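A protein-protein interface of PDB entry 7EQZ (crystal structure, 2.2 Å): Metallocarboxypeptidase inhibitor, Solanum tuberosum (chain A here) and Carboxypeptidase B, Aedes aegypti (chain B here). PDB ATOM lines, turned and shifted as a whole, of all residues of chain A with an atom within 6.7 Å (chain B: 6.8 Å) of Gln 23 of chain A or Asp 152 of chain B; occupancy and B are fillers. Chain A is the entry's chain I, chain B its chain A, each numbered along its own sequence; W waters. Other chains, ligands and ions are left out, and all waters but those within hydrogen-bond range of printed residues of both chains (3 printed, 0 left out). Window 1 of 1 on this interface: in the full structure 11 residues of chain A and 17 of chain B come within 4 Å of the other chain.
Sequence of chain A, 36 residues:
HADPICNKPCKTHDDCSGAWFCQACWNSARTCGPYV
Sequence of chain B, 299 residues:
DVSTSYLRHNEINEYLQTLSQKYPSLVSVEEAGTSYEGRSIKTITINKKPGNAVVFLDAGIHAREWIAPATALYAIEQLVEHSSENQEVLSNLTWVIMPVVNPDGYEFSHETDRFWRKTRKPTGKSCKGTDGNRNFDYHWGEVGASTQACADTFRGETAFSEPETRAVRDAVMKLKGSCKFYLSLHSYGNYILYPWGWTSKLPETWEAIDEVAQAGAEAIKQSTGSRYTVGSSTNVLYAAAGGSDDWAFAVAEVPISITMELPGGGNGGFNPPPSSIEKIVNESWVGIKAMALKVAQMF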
ATOM      1  N   ASP A   3      16.568   0.956  11.377  1.00  0.00           N
ATOM      2  CA  ASP A   3      15.969   2.235  11.749  1.00  0.00           C
ATOM      3  C   ASP A   3      16.307   3.281  10.694  1.00  0.00           C
ATOM      4  O   ASP A   3      17.432   3.803  10.676  1.00  0.00           O
ATOM      5  CB  ASP A   3      16.465   2.681  13.127  1.00  0.00           C
ATOM      6  CG  ASP A   3      15.733   3.903  13.644  1.00  0.00           C
ATOM      7  OD1 ASP A   3      14.743   4.325  13.009  1.00  0.00           O
ATOM      8  OD2 ASP A   3      16.147   4.443  14.690  1.00  0.00           O
ATOM      9  N   ILE A   5      15.541   6.332  10.475  1.00  0.00           N
ATOM     10  CA  ILE A   5      15.795   7.655  11.040  1.00  0.00           C
ATOM     11  C   ILE A   5      17.238   7.834  11.485  1.00  0.00           C
ATOM     12  O   ILE A   5      17.673   8.967  11.718  1.00  0.00           O
ATOM     13  CB  ILE A   5      14.828   7.915  12.215  1.00  0.00           C
ATOM     14  CG1 ILE A   5      13.417   7.463  11.846  1.00  0.00           C
ATOM     15  CG2 ILE A   5      14.801   9.391  12.591  1.00  0.00           C
ATOM     16  CD1 ILE A   5      12.761   8.336  10.800  1.00  0.00           C
ATOM     17  N   CYS A   6      17.995   6.749  11.610  1.00  0.00           N
ATOM     18  CA  CYS A   6      19.396   6.865  11.989  1.00  0.00           C
ATOM     19  C   CYS A   6      20.173   7.629  10.925  1.00  0.00           C
ATOM     20  O   CYS A   6      20.004   7.400   9.724  1.00  0.00           O
ATOM     21  CB  CYS A   6      20.006   5.479  12.202  1.00  0.00           C
ATOM     22  SG  CYS A   6      19.432   4.639  13.697  1.00  0.00           S
ATOM     23  N   THR A  12      16.705  19.599  16.168  1.00  0.00           N
ATOM     24  CA  THR A  12      16.188  19.321  17.499  1.00  0.00           C
ATOM     25  C   THR A  12      15.780  17.855  17.573  1.00  0.00           C
ATOM     26  O   THR A  12      15.821  17.125  16.581  1.00  0.00           O
ATOM     27  CB  THR A  12      14.995  20.223  17.845  1.00  0.00           C
ATOM     28  OG1 THR A  12      14.025  20.161  16.792  1.00  0.00           O
ATOM     29  CG2 THR A  12      15.449  21.663  18.029  1.00  0.00           C
ATOM     30  N   HIS A  13      15.379  17.427  18.772  1.00  0.00           N
ATOM     31  CA  HIS A  13      14.987  16.035  18.962  1.00  0.00           C
ATOM     32  C   HIS A  13      13.709  15.694  18.207  1.00  0.00           C
ATOM     33  O   HIS A  13      13.490  14.525  17.867  1.00  0.00           O
ATOM     34  CB  HIS A  13      14.818  15.735  20.451  1.00  0.00           C
ATOM     35  CG  HIS A  13      16.086  15.858  21.239  1.00  0.00           C
ATOM     36  ND1 HIS A  13      17.156  15.008  21.063  1.00  0.00           N
ATOM     37  CD2 HIS A  13      16.455  16.731  22.206  1.00  0.00           C
ATOM     38  CE1 HIS A  13      18.130  15.351  21.889  1.00  0.00           C
ATOM     39  NE2 HIS A  13      17.729  16.394  22.593  1.00  0.00           N
ATOM     40  N   ASP A  14      12.860  16.689  17.931  1.00  0.00           N
ATOM     41  CA  ASP A  14      11.614  16.424  17.219  1.00  0.00           C
ATOM     42  C   ASP A  14      11.866  15.937  15.798  1.00  0.00           C
ATOM     43  O   ASP A  14      11.035  15.213  15.237  1.00  0.00           O
ATOM     44  CB  ASP A  14      10.740  17.678  17.207  1.00  0.00           C
ATOM     45  N   CYS A  16      13.886  13.738  15.029  1.00  0.00           N
ATOM     46  CA  CYS A  16      14.127  12.308  15.153  1.00  0.00           C
ATOM     47  C   CYS A  16      12.905  11.557  15.671  1.00  0.00           C
ATOM     48  O   CYS A  16      13.035  10.421  16.139  1.00  0.00           O
ATOM     49  CB  CYS A  16      15.331  12.050  16.061  1.00  0.00           C
ATOM     50  SG  CYS A  16      16.804  13.024  15.663  1.00  0.00           S
ATOM     51  N   SER A  17      11.725  12.169  15.606  1.00  0.00           N
ATOM     52  CA  SER A  17      10.515  11.530  16.102  1.00  0.00           C
ATOM     53  C   SER A  17      10.179  10.290  15.281  1.00  0.00           C
ATOM     54  O   SER A  17      10.416  10.233  14.071  1.00  0.00           O
ATOM     55  CB  SER A  17       9.342  12.509  16.072  1.00  0.00           C
ATOM     56  OG  SER A  17       9.151  13.035  14.769  1.00  0.00           O
ATOM     57  N   GLY A  18       9.615   9.293  15.954  1.00  0.00           N
ATOM     58  CA  GLY A  18       9.299   8.031  15.307  1.00  0.00           C
ATOM     59  C   GLY A  18      10.514   7.246  14.862  1.00  0.00           C
ATOM     60  O   GLY A  18      10.529   6.718  13.742  1.00  0.00           O
ATOM     61  N   ALA A  19      11.534   7.154  15.710  1.00  0.00           N
ATOM     62  CA  ALA A  19      12.780   6.475  15.376  1.00  0.00           C
ATOM     63  C   ALA A  19      12.976   5.159  16.109  1.00  0.00           C
ATOM     64  O   ALA A  19      13.524   4.225  15.533  1.00  0.00           O
ATOM     65  CB  ALA A  19      13.974   7.388  15.672  1.00  0.00           C
ATOM     66  N   TRP A  20      12.636   5.112  17.397  1.00  0.00           N
ATOM     67  CA  TRP A  20      12.649   3.944  18.280  1.00  0.00           C
ATOM     68  C   TRP A  20      14.058   3.449  18.584  1.00  0.00           C
ATOM     69  O   TRP A  20      14.262   2.753  19.585  1.00  0.00           O
ATOM     70  CB  TRP A  20      11.794   2.792  17.707  1.00  0.00           C
ATOM     71  CG  TRP A  20      12.454   1.854  16.685  1.00  0.00           C
ATOM     72  CD1 TRP A  20      12.235   1.840  15.335  1.00  0.00           C
ATOM     73  CD2 TRP A  20      13.385   0.784  16.942  1.00  0.00           C
ATOM     74  NE1 TRP A  20      12.986   0.862  14.737  1.00  0.00           N
ATOM     75  CE2 TRP A  20      13.698   0.196  15.699  1.00  0.00           C
ATOM     76  CE3 TRP A  20      13.989   0.275  18.096  1.00  0.00           C
ATOM     77  CZ2 TRP A  20      14.587  -0.871  15.579  1.00  0.00           C
ATOM     78  CZ3 TRP A  20      14.874  -0.783  17.974  1.00  0.00           C
ATOM     79  CH2 TRP A  20      15.163  -1.344  16.725  1.00  0.00           C
ATOM     80  N   PHE A  21      15.049   3.845  17.786  1.00  0.00           N
ATOM     81  CA  PHE A  21      16.434   3.534  18.121  1.00  0.00           C
ATOM     82  C   PHE A  21      17.281   4.799  18.141  1.00  0.00           C
ATOM     83  O   PHE A  21      17.979   5.075  19.121  1.00  0.00           O
ATOM     84  CB  PHE A  21      17.012   2.516  17.137  1.00  0.00           C
ATOM     85  CG  PHE A  21      18.413   2.084  17.467  1.00  0.00           C
ATOM     86  CD1 PHE A  21      18.653   1.212  18.515  1.00  0.00           C
ATOM     87  CD2 PHE A  21      19.490   2.551  16.730  1.00  0.00           C
ATOM     88  CE1 PHE A  21      19.940   0.814  18.824  1.00  0.00           C
ATOM     89  CE2 PHE A  21      20.780   2.156  17.034  1.00  0.00           C
ATOM     90  CZ  PHE A  21      21.005   1.287  18.083  1.00  0.00           C
ATOM     91  N   CYS A  22      17.210   5.573  17.062  1.00  0.00           N
ATOM     92  CA  CYS A  22      17.970   6.815  16.931  1.00  0.00           C
ATOM     93  C   CYS A  22      17.083   8.016  17.259  1.00  0.00           C
ATOM     94  O   CYS A  22      16.813   8.878  16.423  1.00  0.00           O
ATOM     95  CB  CYS A  22      18.561   6.924  15.527  1.00  0.00           C
ATOM     96  SG  CYS A  22      20.000   5.858  15.222  1.00  0.00           S
ATOM     97  N   GLN A  23      16.631   8.058  18.512  1.00  0.00           N
ATOM     98  CA  GLN A  23      15.693   9.080  18.957  1.00  0.00           C
ATOM     99  C   GLN A  23      16.366  10.385  19.359  1.00  0.00           C
ATOM    100  O   GLN A  23      15.668  11.383  19.563  1.00  0.00           O
ATOM    101  CB  GLN A  23      14.870   8.556  20.137  1.00  0.00           C
ATOM    102  CG  GLN A  23      14.470   7.098  20.021  1.00  0.00           C
ATOM    103  CD  GLN A  23      13.727   6.603  21.246  1.00  0.00           C
ATOM    104  OE1 GLN A  23      14.241   5.785  22.009  1.00  0.00           O
ATOM    105  NE2 GLN A  23      12.512   7.100  21.442  1.00  0.00           N
ATOM    106  N   ALA A  24      17.689  10.407  19.476  1.00  0.00           N
ATOM    107  CA  ALA A  24      18.410  11.571  19.972  1.00  0.00           C
ATOM    108  C   ALA A  24      19.063  12.319  18.817  1.00  0.00           C
ATOM    109  O   ALA A  24      19.672  11.704  17.936  1.00  0.00           O
ATOM    110  CB  ALA A  24      19.469  11.160  20.997  1.00  0.00           C
ATOM    111  N   CYS A  25      18.931  13.643  18.826  1.00  0.00           N
ATOM    112  CA  CYS A  25      19.622  14.500  17.870  1.00  0.00           C
ATOM    113  C   CYS A  25      20.960  14.907  18.475  1.00  0.00           C
ATOM    114  O   CYS A  25      21.005  15.694  19.426  1.00  0.00           O
ATOM    115  CB  CYS A  25      18.780  15.725  17.527  1.00  0.00           C
ATOM    116  SG  CYS A  25      19.515  16.783  16.255  1.00  0.00           S
ATOM    117  N   CYS A  32      20.532  12.263  13.646  1.00  0.00           N
ATOM    118  CA  CYS A  32      19.819  11.446  14.616  1.00  0.00           C
ATOM    119  C   CYS A  32      20.638  10.211  14.965  1.00  0.00           C
ATOM    120  O   CYS A  32      21.116   9.494  14.080  1.00  0.00           O
ATOM    121  CB  CYS A  32      18.453  11.038  14.068  1.00  0.00           C
ATOM    122  SG  CYS A  32      17.314  12.413  13.794  1.00  0.00           S
ATOM    123  N   GLY A  33      20.797   9.962  16.262  1.00  0.00           N
ATOM    124  CA  GLY A  33      21.520   8.809  16.738  1.00  0.00           C
ATOM    125  C   GLY A  33      20.912   8.264  18.012  1.00  0.00           C
ATOM    126  O   GLY A  33      20.032   8.883  18.620  1.00  0.00           O
ATOM    127  N   PRO A  34      21.365   7.091  18.442  1.00  0.00           N
ATOM    128  CA  PRO A  34      20.823   6.501  19.667  1.00  0.00           C
ATOM    129  C   PRO A  34      21.347   7.214  20.903  1.00  0.00           C
ATOM    130  O   PRO A  34      22.332   7.954  20.861  1.00  0.00           O
ATOM    131  CB  PRO A  34      21.318   5.053  19.612  1.00  0.00           C
ATOM    132  CG  PRO A  34      22.595   5.136  18.841  1.00  0.00           C
ATOM    133  CD  PRO A  34      22.437   6.269  17.854  1.00  0.00           C
ATOM    134  N   TYR A  35      20.655   6.991  22.017  1.00  0.00           N
ATOM    135  CA  TYR A  35      21.163   7.448  23.301  1.00  0.00           C
ATOM    136  C   TYR A  35      22.391   6.630  23.675  1.00  0.00           C
ATOM    137  O   TYR A  35      22.368   5.396  23.625  1.00  0.00           O
ATOM    138  CB  TYR A  35      20.085   7.328  24.376  1.00  0.00           C
ATOM    139  CG  TYR A  35      18.964   8.332  24.229  1.00  0.00           C
ATOM    140  CD1 TYR A  35      19.173   9.678  24.499  1.00  0.00           C
ATOM    141  CD2 TYR A  35      17.698   7.934  23.819  1.00  0.00           C
ATOM    142  CE1 TYR A  35      18.152  10.600  24.367  1.00  0.00           C
ATOM    143  CE2 TYR A  35      16.671   8.850  23.684  1.00  0.00           C
ATOM    144  CZ  TYR A  35      16.903  10.181  23.958  1.00  0.00           C
ATOM    145  OH  TYR A  35      15.884  11.096  23.824  1.00  0.00           O
ATOM    146  N   HIS B  62      25.221   1.680  31.160  1.00  0.00           N
ATOM    147  CA  HIS B  62      24.276   1.332  30.109  1.00  0.00           C
ATOM    148  C   HIS B  62      24.657  -0.028  29.544  1.00  0.00           C
ATOM    149  O   HIS B  62      25.827  -0.270  29.227  1.00  0.00           O
ATOM    150  CB  HIS B  62      24.257   2.399  29.014  1.00  0.00           C
ATOM    151  CG  HIS B  62      23.684   3.708  29.461  1.00  0.00           C
ATOM    152  ND1 HIS B  62      24.305   4.914  29.224  1.00  0.00           N
ATOM    153  CD2 HIS B  62      22.548   3.997  30.140  1.00  0.00           C
ATOM    154  CE1 HIS B  62      23.575   5.892  29.732  1.00  0.00           C
ATOM    155  NE2 HIS B  62      22.503   5.361  30.292  1.00  0.00           N
ATOM    156  N   ARG B  64      24.144  -1.989  26.793  1.00  0.00           N
ATOM    157  CA  ARG B  64      24.629  -2.331  25.459  1.00  0.00           C
ATOM    158  C   ARG B  64      26.015  -1.781  25.159  1.00  0.00           C
ATOM    159  O   ARG B  64      26.586  -2.133  24.121  1.00  0.00           O
ATOM    160  CB  ARG B  64      23.645  -1.832  24.402  1.00  0.00           C
ATOM    161  CG  ARG B  64      23.313  -0.355  24.515  1.00  0.00           C
ATOM    162  CD  ARG B  64      22.036  -0.033  23.762  1.00  0.00           C
ATOM    163  NE  ARG B  64      21.746   1.395  23.743  1.00  0.00           N
ATOM    164  CZ  ARG B  64      20.659   1.925  23.201  1.00  0.00           C
ATOM    165  NH1 ARG B  64      19.735   1.173  22.627  1.00  0.00           N
ATOM    166  NH2 ARG B  64      20.495   3.245  23.234  1.00  0.00           N
ATOM    167  N   PHE B 115      20.695  -4.774  22.610  1.00  0.00           N
ATOM    168  CA  PHE B 115      20.650  -3.318  22.647  1.00  0.00           C
ATOM    169  C   PHE B 115      19.804  -2.791  23.803  1.00  0.00           C
ATOM    170  O   PHE B 115      19.233  -1.701  23.718  1.00  0.00           O
ATOM    171  CB  PHE B 115      20.151  -2.777  21.308  1.00  0.00           C
ATOM    172  CG  PHE B 115      21.056  -3.117  20.158  1.00  0.00           C
ATOM    173  CD1 PHE B 115      22.187  -2.360  19.903  1.00  0.00           C
ATOM    174  CD2 PHE B 115      20.791  -4.209  19.349  1.00  0.00           C
ATOM    175  CE1 PHE B 115      23.028  -2.676  18.853  1.00  0.00           C
ATOM    176  CE2 PHE B 115      21.628  -4.530  18.296  1.00  0.00           C
ATOM    177  CZ  PHE B 115      22.749  -3.762  18.048  1.00  0.00           C
ATOM    178  N   ARG B 117      19.482  -0.978  27.358  1.00  0.00           N
ATOM    179  CA  ARG B 117      20.250   0.147  27.878  1.00  0.00           C
ATOM    180  C   ARG B 117      20.106   0.347  29.378  1.00  0.00           C
ATOM    181  O   ARG B 117      21.109   0.567  30.063  1.00  0.00           O
ATOM    182  CB  ARG B 117      19.838   1.436  27.144  1.00  0.00           C
ATOM    183  CG  ARG B 117      20.118   2.730  27.899  1.00  0.00           C
ATOM    184  CD  ARG B 117      19.497   3.916  27.173  1.00  0.00           C
ATOM    185  NE  ARG B 117      19.822   5.196  27.793  1.00  0.00           N
ATOM    186  CZ  ARG B 117      20.902   5.914  27.511  1.00  0.00           C
ATOM    187  NH1 ARG B 117      21.806   5.490  26.643  1.00  0.00           N
ATOM    188  NH2 ARG B 117      21.078   7.086  28.115  1.00  0.00           N
ATOM    189  N   LYS B 118      18.894   0.251  29.913  1.00  0.00           N
ATOM    190  CA  LYS B 118      18.621   0.659  31.285  1.00  0.00           C
ATOM    191  C   LYS B 118      18.959  -0.469  32.259  1.00  0.00           C
ATOM    192  O   LYS B 118      19.595  -1.467  31.908  1.00  0.00           O
ATOM    193  CB  LYS B 118      17.164   1.096  31.417  1.00  0.00           C
ATOM    194  CG  LYS B 118      16.788   2.271  30.530  1.00  0.00           C
ATOM    195  CD  LYS B 118      15.350   2.704  30.771  1.00  0.00           C
ATOM    196  CE  LYS B 118      14.364   1.694  30.202  1.00  0.00           C
ATOM    197  NZ  LYS B 118      12.957   2.152  30.367  1.00  0.00           N
ATOM    198  N   THR B 130      15.450   1.540  34.395  1.00  0.00           N
ATOM    199  CA  THR B 130      15.652   2.960  34.633  1.00  0.00           C
ATOM    200  C   THR B 130      17.002   3.361  34.056  1.00  0.00           C
ATOM    201  O   THR B 130      17.991   2.640  34.223  1.00  0.00           O
ATOM    202  CB  THR B 130      15.600   3.289  36.135  1.00  0.00           C
ATOM    203  OG1 THR B 130      14.245   3.230  36.599  1.00  0.00           O
ATOM    204  CG2 THR B 130      16.174   4.674  36.414  1.00  0.00           C
ATOM    205  N   ASP B 131      17.042   4.498  33.365  1.00  0.00           N
ATOM    206  CA  ASP B 131      18.303   5.026  32.857  1.00  0.00           C
ATOM    207  C   ASP B 131      19.177   5.431  34.038  1.00  0.00           C
ATOM    208  O   ASP B 131      18.877   6.403  34.739  1.00  0.00           O
ATOM    209  CB  ASP B 131      18.051   6.209  31.925  1.00  0.00           C
ATOM    210  CG  ASP B 131      19.287   6.607  31.130  1.00  0.00           C
ATOM    211  OD1 ASP B 131      20.409   6.215  31.516  1.00  0.00           O
ATOM    212  OD2 ASP B 131      19.136   7.316  30.113  1.00  0.00           O
ATOM    213  N   GLY B 132      20.258   4.680  34.262  1.00  0.00           N
ATOM    214  CA  GLY B 132      21.131   4.972  35.387  1.00  0.00           C
ATOM    215  C   GLY B 132      21.758   6.351  35.304  1.00  0.00           C
ATOM    216  O   GLY B 132      21.943   7.020  36.324  1.00  0.00           O
ATOM    217  N   ARG B 134      20.424   8.962  34.316  1.00  0.00           N
ATOM    218  CA  ARG B 134      19.444   9.994  34.627  1.00  0.00           C
ATOM    219  C   ARG B 134      18.928   9.852  36.053  1.00  0.00           C
ATOM    220  O   ARG B 134      17.909  10.458  36.400  1.00  0.00           O
ATOM    221  CB  ARG B 134      18.269   9.948  33.643  1.00  0.00           C
ATOM    222  CG  ARG B 134      18.666   9.927  32.176  1.00  0.00           C
ATOM    223  CD  ARG B 134      19.157  11.287  31.705  1.00  0.00           C
ATOM    224  NE  ARG B 134      19.389  11.308  30.266  1.00  0.00           N
ATOM    225  CZ  ARG B 134      20.428  10.742  29.664  1.00  0.00           C
ATOM    226  NH1 ARG B 134      21.366  10.110  30.352  1.00  0.00           N
ATOM    227  NH2 ARG B 134      20.528  10.813  28.340  1.00  0.00           N
ATOM    228  N   SER B 146      13.320  11.527  30.899  1.00  0.00           N
ATOM    229  CA  SER B 146      11.920  11.269  30.601  1.00  0.00           C
ATOM    230  C   SER B 146      11.184  10.809  31.851  1.00  0.00           C
ATOM    231  O   SER B 146      11.735  10.069  32.673  1.00  0.00           O
ATOM    232  CB  SER B 146      11.776  10.215  29.503  1.00  0.00           C
ATOM    233  OG  SER B 146      10.418   9.851  29.330  1.00  0.00           O
ATOM    234  N   GLN B 148       8.479   9.019  31.451  1.00  0.00           N
ATOM    235  CA  GLN B 148       7.803   7.811  30.997  1.00  0.00           C
ATOM    236  C   GLN B 148       8.661   6.590  31.302  1.00  0.00           C
ATOM    237  O   GLN B 148       9.845   6.550  30.949  1.00  0.00           O
ATOM    238  CB  GLN B 148       7.498   7.892  29.502  1.00  0.00           C
ATOM    239  CG  GLN B 148       6.744   9.150  29.098  1.00  0.00           C
ATOM    240  CD  GLN B 148       5.448   9.318  29.870  1.00  0.00           C
ATOM    241  OE1 GLN B 148       5.352  10.149  30.773  1.00  0.00           O
ATOM    242  NE2 GLN B 148       4.443   8.525  29.517  1.00  0.00           N
ATOM    243  N   ALA B 149       8.055   5.597  31.954  1.00  0.00           N
ATOM    244  CA  ALA B 149       8.810   4.440  32.421  1.00  0.00           C
ATOM    245  C   ALA B 149       9.369   3.619  31.267  1.00  0.00           C
ATOM    246  O   ALA B 149      10.371   2.915  31.438  1.00  0.00           O
ATOM    247  CB  ALA B 149       7.926   3.571  33.314  1.00  0.00           C
ATOM    248  N   CYS B 150       8.748   3.692  30.090  1.00  0.00           N
ATOM    249  CA  CYS B 150       9.169   2.898  28.944  1.00  0.00           C
ATOM    250  C   CYS B 150      10.229   3.581  28.087  1.00  0.00           C
ATOM    251  O   CYS B 150      10.729   2.961  27.144  1.00  0.00           O
ATOM    252  CB  CYS B 150       7.956   2.553  28.074  1.00  0.00           C
ATOM    253  SG  CYS B 150       6.754   1.489  28.897  1.00  0.00           S
ATOM    254  N   ALA B 151      10.580   4.827  28.385  1.00  0.00           N
ATOM    255  CA  ALA B 151      11.543   5.551  27.570  1.00  0.00           C
ATOM    256  C   ALA B 151      12.969   5.100  27.875  1.00  0.00           C
ATOM    257  O   ALA B 151      13.271   4.583  28.954  1.00  0.00           O
ATOM    258  CB  ALA B 151      11.411   7.056  27.793  1.00  0.00           C
ATOM    259  N   ASP B 152      13.853   5.311  26.896  1.00  0.00           N
ATOM    260  CA  ASP B 152      15.262   4.980  27.076  1.00  0.00           C
ATOM    261  C   ASP B 152      15.902   5.816  28.174  1.00  0.00           C
ATOM    262  O   ASP B 152      16.862   5.373  28.815  1.00  0.00           O
ATOM    263  CB  ASP B 152      16.023   5.180  25.765  1.00  0.00           C
ATOM    264  CG  ASP B 152      15.732   4.101  24.745  1.00  0.00           C
ATOM    265  OD1 ASP B 152      14.905   3.211  25.039  1.00  0.00           O
ATOM    266  OD2 ASP B 152      16.326   4.144  23.648  1.00  0.00           O
ATOM    267  N   THR B 153      15.390   7.025  28.405  1.00  0.00           N
ATOM    268  CA  THR B 153      15.966   7.958  29.363  1.00  0.00           C
ATOM    269  C   THR B 153      15.075   8.146  30.587  1.00  0.00           C
ATOM    270  O   THR B 153      15.005   9.243  31.147  1.00  0.00           O
ATOM    271  CB  THR B 153      16.234   9.306  28.697  1.00  0.00           C
ATOM    272  OG1 THR B 153      14.996   9.869  28.245  1.00  0.00           O
ATOM    273  CG2 THR B 153      17.167   9.133  27.506  1.00  0.00           C
ATOM    274  N   PHE B 154      14.391   7.086  31.012  1.00  0.00           N
ATOM    275  CA  PHE B 154      13.513   7.180  32.173  1.00  0.00           C
ATOM    276  C   PHE B 154      14.313   7.554  33.413  1.00  0.00           C
ATOM    277  O   PHE B 154      15.279   6.872  33.772  1.00  0.00           O
ATOM    278  CB  PHE B 154      12.778   5.857  32.389  1.00  0.00           C
ATOM    279  CG  PHE B 154      11.890   5.848  33.602  1.00  0.00           C
ATOM    280  CD1 PHE B 154      11.046   6.915  33.867  1.00  0.00           C
ATOM    281  CD2 PHE B 154      11.900   4.774  34.477  1.00  0.00           C
ATOM    282  CE1 PHE B 154      10.228   6.912  34.982  1.00  0.00           C
ATOM    283  CE2 PHE B 154      11.084   4.764  35.594  1.00  0.00           C
ATOM    284  CZ  PHE B 154      10.248   5.835  35.847  1.00  0.00           C
HETATM  285  O   HOH W   1      23.113   3.551  25.205  1.00  0.00           O
HETATM  286  O   HOH W   2      12.729   5.906  24.357  1.00  0.00           O
HETATM  287  O   HOH W   3      18.449   4.853  21.858  1.00  0.00           O
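Water W1 lies within hydrogen-bond range of O of Tyr 35 of chain A (2.5 Å), NH1 of Arg 117 of chain B (2.7 Å) and NE of Arg 64 of chain B (2.9 Å). Water W3 lies within hydrogen-bond range of the backbone carbonyl oxygen of Phe 21 of chain A (2.8 Å), the side-chain carboxylate of Asp 152 of chain B (2.9 Å), the guanidinium group of Arg 64 of chain B (2.9 Å) and the backbone NH of Tyr 35 of chain A (3.1 Å). Water W2 lies within hydrogen-bond range of OE1 of Gln 23 of chain A and N of Asp 152 of chain B.
A ring nitrogen (NE2) of His 62 of chain B lies within hydrogen-bond range of the guanidinium group (NH2) of Arg 117 of chain B (3.1 Å). The guanidinium group (NH2) of Arg 117 of chain B lies within salt-bridge range of the side-chain carboxylate (OD2) of Asp 131 of chain B, at 2.8 Å. The guanidinium group (NE) of Arg 117 of chain B lies within hydrogen-bond range of the backbone carbonyl oxygen (O) of Asp 152 of chain B (3.1 Å). The backbone NH (N) of Ser 146 of chain B lies within hydrogen-bond range of the backbone carbonyl oxygen (O) of Thr 153 of chain B (2.8 Å). The backbone NH of Phe 21 of chain A lies close to the side-chain carboxylate of Asp 3 of chain A (3.3 Å). The side-chain sulfur (SG) of Cys 6 of chain A is disulfide-bonded to the side-chain sulfur (SG) of Cys 22 of chain A.
Of the 20 printed residues of chain A, 3 touch a printed residue of chain B. Along chain A the printed residues that touch a printed residue of chain B span positions 21 to 35. Printed residues of chain B that touch a printed residue of chain A: Arg 64, Arg 117, Asp 152 and Thr 153.
NH2 of Arg 64 of chain B sits at hydrogen-bond distance from O of Tyr 35 of chain A, 2.9 Å away. The backbone carbonyl oxygen (O) of Tyr 35 of chain A lies within hydrogen-bond range of the guanidinium group (NH1) of Arg 117 of chain B. OE1 of Gln 23 of chain A lies close to OD2 of Asp 152 of chain B.
Gln 23 of chain A touches one residue of chain B. Asp 152 of chain B touches just these residues of chain A: Gln 23 and Tyr 35. Of the printed residues of chain A, Thr 153 of chain B touches Tyr 35. Printed residues of chain B within 4 Å of Tyr 35 of chain A: Arg 64, Arg 117, Asp 152 and Thr 153. Printed residues of chain A within 4 Å of Arg 117 of chain B: Tyr 35 (3.1 Å). Of the printed residues of chain B, Phe 21 of chain A touches Arg 64 (3.8 Å). Printed residues of chain A within 4 Å of Arg 64 of chain B: Phe 21 and Tyr 35. Thr 130 of chain B touches none of the printed residues of chain A. Ala 151 of chain B touches none of the printed residues of chain A.
Among the printed residues, pairs that only touch across the chains: Tyr 35 of chain A with Thr 153 of chain B (3.6 Å), Tyr 35 of chain A with Asp 152 of chain B (3.8 Å) and Phe 21 of chain A with Arg 64 of chain B (3.8 Å).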
